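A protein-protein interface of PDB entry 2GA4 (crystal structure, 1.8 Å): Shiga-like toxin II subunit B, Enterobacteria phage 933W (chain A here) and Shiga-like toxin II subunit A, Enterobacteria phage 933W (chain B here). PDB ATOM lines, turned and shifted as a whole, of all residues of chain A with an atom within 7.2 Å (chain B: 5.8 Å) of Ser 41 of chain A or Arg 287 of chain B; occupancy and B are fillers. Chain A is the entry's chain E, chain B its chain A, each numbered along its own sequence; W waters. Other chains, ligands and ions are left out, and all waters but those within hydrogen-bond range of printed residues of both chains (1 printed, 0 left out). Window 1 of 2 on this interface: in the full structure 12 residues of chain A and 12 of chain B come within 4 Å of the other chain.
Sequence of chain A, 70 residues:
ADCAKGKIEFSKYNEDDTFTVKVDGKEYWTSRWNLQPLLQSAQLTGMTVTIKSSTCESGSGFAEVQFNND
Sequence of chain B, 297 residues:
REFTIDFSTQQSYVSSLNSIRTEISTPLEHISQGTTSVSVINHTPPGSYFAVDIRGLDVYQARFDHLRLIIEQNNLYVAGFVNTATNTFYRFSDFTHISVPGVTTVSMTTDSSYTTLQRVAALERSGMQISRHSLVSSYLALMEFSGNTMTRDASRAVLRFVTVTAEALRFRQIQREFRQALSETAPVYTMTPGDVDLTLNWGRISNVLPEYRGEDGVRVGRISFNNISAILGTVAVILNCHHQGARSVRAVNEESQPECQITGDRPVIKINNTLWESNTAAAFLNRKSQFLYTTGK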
ATOM      1  N   ILE A   8      11.944  -4.678  16.942  1.00  0.00           N
ATOM      2  CA  ILE A   8      12.258  -6.081  16.824  1.00  0.00           C
ATOM      3  C   ILE A   8      12.616  -6.403  15.392  1.00  0.00           C
ATOM      4  O   ILE A   8      11.818  -6.193  14.489  1.00  0.00           O
ATOM      5  CB  ILE A   8      11.063  -6.940  17.297  1.00  0.00           C
ATOM      6  CG1 ILE A   8      10.865  -6.706  18.796  1.00  0.00           C
ATOM      7  CG2 ILE A   8      11.327  -8.416  16.984  1.00  0.00           C
ATOM      8  CD1 ILE A   8       9.557  -7.269  19.283  1.00  0.00           C
ATOM      9  N   LEU A  35       4.168 -13.338  26.302  1.00  0.00           N
ATOM     10  CA  LEU A  35       4.942 -12.380  25.548  1.00  0.00           C
ATOM     11  C   LEU A  35       4.918 -12.593  24.052  1.00  0.00           C
ATOM     12  O   LEU A  35       5.296 -11.681  23.293  1.00  0.00           O
ATOM     13  CB  LEU A  35       6.386 -12.396  26.062  1.00  0.00           C
ATOM     14  CG  LEU A  35       6.523 -11.501  27.293  1.00  0.00           C
ATOM     15  CD1 LEU A  35       7.933 -11.743  27.876  1.00  0.00           C
ATOM     16  CD2 LEU A  35       6.404 -10.013  26.918  1.00  0.00           C
ATOM     17  N   GLN A  36       4.454 -13.758  23.596  1.00  0.00           N
ATOM     18  CA  GLN A  36       4.484 -13.940  22.137  1.00  0.00           C
ATOM     19  C   GLN A  36       3.656 -12.970  21.354  1.00  0.00           C
ATOM     20  O   GLN A  36       4.168 -12.294  20.471  1.00  0.00           O
ATOM     21  CB  GLN A  36       4.143 -15.381  21.730  1.00  0.00           C
ATOM     22  CG  GLN A  36       5.282 -16.300  22.239  1.00  0.00           C
ATOM     23  CD  GLN A  36       5.203 -17.710  21.730  1.00  0.00           C
ATOM     24  OE1 GLN A  36       4.632 -17.958  20.689  1.00  0.00           O
ATOM     25  NE2 GLN A  36       5.843 -18.651  22.452  1.00  0.00           N
ATOM     26  N   PRO A  37       2.360 -12.877  21.654  1.00  0.00           N
ATOM     27  CA  PRO A  37       1.576 -11.920  20.867  1.00  0.00           C
ATOM     28  C   PRO A  37       2.026 -10.488  21.133  1.00  0.00           C
ATOM     29  O   PRO A  37       1.951  -9.646  20.259  1.00  0.00           O
ATOM     30  CB  PRO A  37       0.131 -12.172  21.337  1.00  0.00           C
ATOM     31  CG  PRO A  37       0.323 -12.754  22.739  1.00  0.00           C
ATOM     32  CD  PRO A  37       1.526 -13.646  22.591  1.00  0.00           C
ATOM     33  N   LEU A  38       2.418 -10.206  22.365  1.00  0.00           N
ATOM     34  CA  LEU A  38       2.865  -8.845  22.698  1.00  0.00           C
ATOM     35  C   LEU A  38       4.103  -8.484  21.905  1.00  0.00           C
ATOM     36  O   LEU A  38       4.177  -7.407  21.279  1.00  0.00           O
ATOM     37  CB  LEU A  38       3.159  -8.728  24.185  1.00  0.00           C
ATOM     38  CG  LEU A  38       1.935  -9.023  25.071  1.00  0.00           C
ATOM     39  CD1 LEU A  38       2.460  -9.007  26.531  1.00  0.00           C
ATOM     40  CD2 LEU A  38       0.820  -8.003  24.922  1.00  0.00           C
ATOM     41  N   LEU A  39       5.056  -9.400  21.868  1.00  0.00           N
ATOM     42  CA  LEU A  39       6.260  -9.142  21.108  1.00  0.00           C
ATOM     43  C   LEU A  39       6.005  -9.132  19.621  1.00  0.00           C
ATOM     44  O   LEU A  39       6.551  -8.309  18.902  1.00  0.00           O
ATOM     45  CB  LEU A  39       7.305 -10.209  21.417  1.00  0.00           C
ATOM     46  CG  LEU A  39       7.902 -10.100  22.832  1.00  0.00           C
ATOM     47  CD1 LEU A  39       8.685 -11.366  23.111  1.00  0.00           C
ATOM     48  CD2 LEU A  39       8.823  -8.832  22.929  1.00  0.00           C
ATOM     49  N   GLN A  40       5.213 -10.081  19.121  1.00  0.00           N
ATOM     50  CA  GLN A  40       4.978 -10.048  17.691  1.00  0.00           C
ATOM     51  C   GLN A  40       4.212  -8.775  17.295  1.00  0.00           C
ATOM     52  O   GLN A  40       4.513  -8.167  16.261  1.00  0.00           O
ATOM     53  CB  GLN A  40       4.243 -11.291  17.212  1.00  0.00           C
ATOM     54  CG  GLN A  40       4.257 -11.295  15.666  1.00  0.00           C
ATOM     55  CD  GLN A  40       3.171 -12.136  15.096  1.00  0.00           C
ATOM     56  OE1 GLN A  40       2.020 -12.010  15.508  1.00  0.00           O
ATOM     57  NE2 GLN A  40       3.511 -12.989  14.120  1.00  0.00           N
ATOM     58  N   SER A  41       3.210  -8.389  18.083  1.00  0.00           N
ATOM     59  CA  SER A  41       2.496  -7.163  17.788  1.00  0.00           C
ATOM     60  C   SER A  41       3.498  -6.011  17.795  1.00  0.00           C
ATOM     61  O   SER A  41       3.443  -5.163  16.921  1.00  0.00           O
ATOM     62  CB  SER A  41       1.413  -6.920  18.818  1.00  0.00           C
ATOM     63  OG  SER A  41       0.398  -7.884  18.600  1.00  0.00           O
ATOM     64  N   ALA A  42       4.399  -5.986  18.773  1.00  0.00           N
ATOM     65  CA  ALA A  42       5.415  -4.912  18.817  1.00  0.00           C
ATOM     66  C   ALA A  42       6.247  -4.963  17.542  1.00  0.00           C
ATOM     67  O   ALA A  42       6.582  -3.924  16.953  1.00  0.00           O
ATOM     68  CB  ALA A  42       6.351  -5.112  20.058  1.00  0.00           C
ATOM     69  N   GLN A  43       6.603  -6.175  17.112  1.00  0.00           N
ATOM     70  CA  GLN A  43       7.405  -6.290  15.928  1.00  0.00           C
ATOM     71  C   GLN A  43       6.671  -5.758  14.699  1.00  0.00           C
ATOM     72  O   GLN A  43       7.222  -4.957  13.955  1.00  0.00           O
ATOM     73  CB  GLN A  43       7.799  -7.772  15.667  1.00  0.00           C
ATOM     74  CG  GLN A  43       8.529  -7.960  14.341  1.00  0.00           C
ATOM     75  CD  GLN A  43       8.818  -9.430  14.080  1.00  0.00           C
ATOM     76  OE1 GLN A  43       8.485 -10.284  14.917  1.00  0.00           O
ATOM     77  NE2 GLN A  43       9.425  -9.738  12.935  1.00  0.00           N
ATOM     78  N   LEU A  44       5.415  -6.171  14.504  1.00  0.00           N
ATOM     79  CA  LEU A  44       4.749  -5.777  13.279  1.00  0.00           C
ATOM     80  C   LEU A  44       4.274  -4.331  13.247  1.00  0.00           C
ATOM     81  O   LEU A  44       4.018  -3.799  12.178  1.00  0.00           O
ATOM     82  CB  LEU A  44       3.599  -6.744  12.989  1.00  0.00           C
ATOM     83  CG  LEU A  44       2.407  -6.693  13.925  1.00  0.00           C
ATOM     84  CD1 LEU A  44       1.331  -5.764  13.355  1.00  0.00           C
ATOM     85  CD2 LEU A  44       1.821  -8.150  14.038  1.00  0.00           C
ATOM     86  N   THR A  45       4.207  -3.708  14.416  1.00  0.00           N
ATOM     87  CA  THR A  45       3.786  -2.308  14.528  1.00  0.00           C
ATOM     88  C   THR A  45       4.976  -1.383  14.746  1.00  0.00           C
ATOM     89  O   THR A  45       4.804  -0.168  14.876  1.00  0.00           O
ATOM     90  CB  THR A  45       2.829  -2.062  15.704  1.00  0.00           C
ATOM     91  OG1 THR A  45       3.469  -2.454  16.935  1.00  0.00           O
ATOM     92  CG2 THR A  45       1.508  -2.840  15.497  1.00  0.00           C
ATOM     93  N   GLY A  46       6.169  -1.970  14.809  1.00  0.00           N
ATOM     94  CA  GLY A  46       7.377  -1.160  14.947  1.00  0.00           C
ATOM     95  C   GLY A  46       7.556  -0.469  16.286  1.00  0.00           C
ATOM     96  O   GLY A  46       8.177   0.587  16.373  1.00  0.00           O
ATOM     97  N   MET A  47       7.035  -1.062  17.341  1.00  0.00           N
ATOM     98  CA  MET A  47       7.216  -0.486  18.658  1.00  0.00           C
ATOM     99  C   MET A  47       8.664  -0.606  19.061  1.00  0.00           C
ATOM    100  O   MET A  47       9.386  -1.472  18.601  1.00  0.00           O
ATOM    101  CB  MET A  47       6.390  -1.229  19.713  1.00  0.00           C
ATOM    102  CG  MET A  47       4.873  -1.131  19.493  1.00  0.00           C
ATOM    103  SD  MET A  47       4.094  -1.915  20.916  1.00  0.00           S
ATOM    104  CE  MET A  47       3.623  -0.519  21.909  1.00  0.00           C
ATOM    105  N   PHE A  67       7.405  -1.683  26.237  1.00  0.00           N
ATOM    106  CA  PHE A  67       6.925  -1.417  24.903  1.00  0.00           C
ATOM    107  C   PHE A  67       6.623   0.064  24.791  1.00  0.00           C
ATOM    108  O   PHE A  67       5.879   0.592  25.620  1.00  0.00           O
ATOM    109  CB  PHE A  67       5.594  -2.169  24.645  1.00  0.00           C
ATOM    110  CG  PHE A  67       5.711  -3.646  24.766  1.00  0.00           C
ATOM    111  CD1 PHE A  67       5.569  -4.268  26.009  1.00  0.00           C
ATOM    112  CD2 PHE A  67       6.041  -4.422  23.654  1.00  0.00           C
ATOM    113  CE1 PHE A  67       5.759  -5.652  26.147  1.00  0.00           C
ATOM    114  CE2 PHE A  67       6.228  -5.822  23.783  1.00  0.00           C
ATOM    115  CZ  PHE A  67       6.087  -6.431  25.033  1.00  0.00           C
ATOM    116  N   ALA B 283      -3.809  -7.515  12.503  1.00  0.00           N
ATOM    117  CA  ALA B 283      -2.754  -8.373  13.002  1.00  0.00           C
ATOM    118  C   ALA B 283      -2.448  -8.269  14.495  1.00  0.00           C
ATOM    119  O   ALA B 283      -1.739  -9.119  15.004  1.00  0.00           O
ATOM    120  CB  ALA B 283      -1.494  -8.188  12.161  1.00  0.00           C
ATOM    121  N   PHE B 284      -2.920  -7.227  15.179  1.00  0.00           N
ATOM    122  CA  PHE B 284      -2.774  -7.220  16.629  1.00  0.00           C
ATOM    123  C   PHE B 284      -4.168  -7.304  17.280  1.00  0.00           C
ATOM    124  O   PHE B 284      -4.274  -7.327  18.486  1.00  0.00           O
ATOM    125  CB  PHE B 284      -1.951  -6.040  17.166  1.00  0.00           C
ATOM    126  CG  PHE B 284      -2.523  -4.689  16.882  1.00  0.00           C
ATOM    127  CD1 PHE B 284      -3.497  -4.152  17.697  1.00  0.00           C
ATOM    128  CD2 PHE B 284      -2.000  -3.910  15.849  1.00  0.00           C
ATOM    129  CE1 PHE B 284      -3.959  -2.839  17.517  1.00  0.00           C
ATOM    130  CE2 PHE B 284      -2.448  -2.589  15.652  1.00  0.00           C
ATOM    131  CZ  PHE B 284      -3.431  -2.049  16.488  1.00  0.00           C
ATOM    132  N   LEU B 285      -5.236  -7.352  16.478  1.00  0.00           N
ATOM    133  CA  LEU B 285      -6.575  -7.509  17.048  1.00  0.00           C
ATOM    134  C   LEU B 285      -7.072  -8.950  16.809  1.00  0.00           C
ATOM    135  O   LEU B 285      -8.261  -9.237  16.923  1.00  0.00           O
ATOM    136  CB  LEU B 285      -7.568  -6.526  16.404  1.00  0.00           C
ATOM    137  CG  LEU B 285      -7.148  -5.079  16.588  1.00  0.00           C
ATOM    138  CD1 LEU B 285      -8.057  -4.153  15.795  1.00  0.00           C
ATOM    139  CD2 LEU B 285      -7.206  -4.749  18.095  1.00  0.00           C
ATOM    140  N   ASN B 286      -6.179  -9.862  16.455  1.00  0.00           N
ATOM    141  CA  ASN B 286      -6.617 -11.221  16.217  1.00  0.00           C
ATOM    142  C   ASN B 286      -6.180 -12.138  17.355  1.00  0.00           C
ATOM    143  O   ASN B 286      -6.108 -13.347  17.157  1.00  0.00           O
ATOM    144  CB  ASN B 286      -6.056 -11.749  14.893  1.00  0.00           C
ATOM    145  CG  ASN B 286      -4.532 -11.865  14.919  1.00  0.00           C
ATOM    146  OD1 ASN B 286      -3.905 -11.393  15.866  1.00  0.00           O
ATOM    147  ND2 ASN B 286      -3.939 -12.459  13.883  1.00  0.00           N
ATOM    148  N   ARG B 287      -5.902 -11.582  18.530  1.00  0.00           N
ATOM    149  CA  ARG B 287      -5.482 -12.425  19.641  1.00  0.00           C
ATOM    150  C   ARG B 287      -6.674 -12.835  20.472  1.00  0.00           C
ATOM    151  O   ARG B 287      -7.585 -12.045  20.678  1.00  0.00           O
ATOM    152  CB  ARG B 287      -4.531 -11.689  20.550  1.00  0.00           C
ATOM    153  CG  ARG B 287      -3.104 -11.564  20.011  1.00  0.00           C
ATOM    154  CD  ARG B 287      -2.943 -10.541  18.890  1.00  0.00           C
ATOM    155  NE  ARG B 287      -1.500 -10.379  18.640  1.00  0.00           N
ATOM    156  CZ  ARG B 287      -0.810 -10.959  17.663  1.00  0.00           C
ATOM    157  NH1 ARG B 287      -1.382 -11.779  16.776  1.00  0.00           N
ATOM    158  NH2 ARG B 287       0.513 -10.728  17.576  1.00  0.00           N
ATOM    159  N   LYS B 288      -6.677 -14.066  20.965  1.00  0.00           N
ATOM    160  CA  LYS B 288      -7.802 -14.408  21.826  1.00  0.00           C
ATOM    161  C   LYS B 288      -7.432 -13.980  23.267  1.00  0.00           C
ATOM    162  O   LYS B 288      -6.411 -13.367  23.520  1.00  0.00           O
ATOM    163  CB  LYS B 288      -8.095 -15.903  21.818  1.00  0.00           C
ATOM    164  CG  LYS B 288      -7.009 -16.740  22.427  1.00  0.00           C
ATOM    165  CD  LYS B 288      -7.473 -18.244  22.358  1.00  0.00           C
ATOM    166  CE  LYS B 288      -6.383 -19.169  22.927  1.00  0.00           C
ATOM    167  NZ  LYS B 288      -6.723 -20.624  22.764  1.00  0.00           N
ATOM    168  N   SER B 289      -8.307 -14.286  24.201  1.00  0.00           N
ATOM    169  CA  SER B 289      -8.072 -13.960  25.607  1.00  0.00           C
ATOM    170  C   SER B 289      -6.712 -14.470  26.025  1.00  0.00           C
ATOM    171  O   SER B 289      -6.376 -15.647  25.844  1.00  0.00           O
ATOM    172  CB  SER B 289      -9.151 -14.627  26.445  1.00  0.00           C
ATOM    173  OG  SER B 289      -8.763 -14.606  27.800  1.00  0.00           O
HETATM  174  O   HOH W   1      -1.025  -8.238  20.899  1.00  0.00           O
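NH2 of Arg 287 of chain B sits at hydrogen-bond distance from O of Pro 37 of chain A, 3.2 Å away.
The guanidinium group (NH2) of Arg 287 of chain B is in hydrogen-bond range of the side-chain amide oxygen (OE1) of Gln 40 of chain A (2.9 Å).
The guanidinium group (NH2) of Arg 287 of chain B sits at hydrogen-bond distance from the side-chain hydroxyl (OG) of Ser 41 of chain A, at 3.0 Å.
The guanidinium group (NH1) of Arg 287 of chain B is in hydrogen-bond range of the side-chain amide oxygen (OD1) of Asn 286 of chain B, 2.7 Å away.
The backbone carbonyl oxygen of Ala 42 of chain A sits at hydrogen-bond distance from the side-chain hydroxyl of Thr 45 of chain A (3.4 Å).
The side-chain hydroxyl (OG) of Ser 41 of chain A is in hydrogen-bond range of the backbone carbonyl oxygen (O) of Pro 37 of chain A, at 2.9 Å.
O of Ala 283 of chain B sits close to OD1 of Asn 286 of chain B (3.3 Å).
The backbone carbonyl oxygen of Ala 283 of chain B is in hydrogen-bond range of the guanidinium group of Arg 287 of chain B (3.2 Å).
The backbone carbonyl oxygen (O) of Ser 41 of chain A sits at hydrogen-bond distance from the side-chain hydroxyl (OG1) of Thr 45 of chain A, at 2.7 Å.
Ser 41 of chain A touches Phe 284 of chain B (OG to CB, 3.3 Å).
Leu 44 of chain A touches Ala 283 of chain B (CD2 to CB, 3.8 Å).
Thr 45 of chain A touches Phe 284 of chain B.
Of chain B, only Phe 284 (3.3 Å) and Arg 287 (3.0 Å) come within 4 Å of Ser 41 of chain A.
Arg 287 of chain B touches three residues of chain A.
Of the printed residues of chain A, Ala 283 of chain B touches Leu 44 (3.8 Å).
Of the printed residues of chain B, Pro 37 of chain A touches Arg 287.
Printed residues of chain B within 4 Å of Gln 40 of chain A: Arg 287.
Printed residues of chain B within 4 Å of Thr 45 of chain A: Phe 284 (3.7 Å).
Of the printed residues of chain A, Phe 284 of chain B touches Ser 41 (3.3 Å) and Thr 45 (3.7 Å).
Leu 38 of chain A touches none of the printed residues of chain B.
The nearest residue of chain B that does not touch Ser 41 of chain A is Ala 283 of chain B (4.4 Å).
The nearest residue of chain A that does not touch Arg 287 of chain B is Leu 44 of chain A (4.6 Å).
Printed residues of chain B that touch a printed residue of chain A: Ala 283, Phe 284 and Arg 287.
Hydrophobic or aromatic side chains of chain B that line the printed part of chain A: Ala 283 and Phe 284.
Of the 15 printed residues of chain A, 5 touch a printed residue of chain B.
Printed residues of chain A that touch a printed residue of chain B: Pro 37, Gln 40, Ser 41, Leu 44 and Thr 45.
Hydrophobic or aromatic side chains of chain A that line the printed part of chain B: Pro 37 and Leu 44.
Water W1 lies within hydrogen-bond range of OG of Ser 41 of chain A (2.7 Å), NE of Arg 287 of chain B (3.1 Å) and O of Pro 37 of chain A (3.4 Å).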
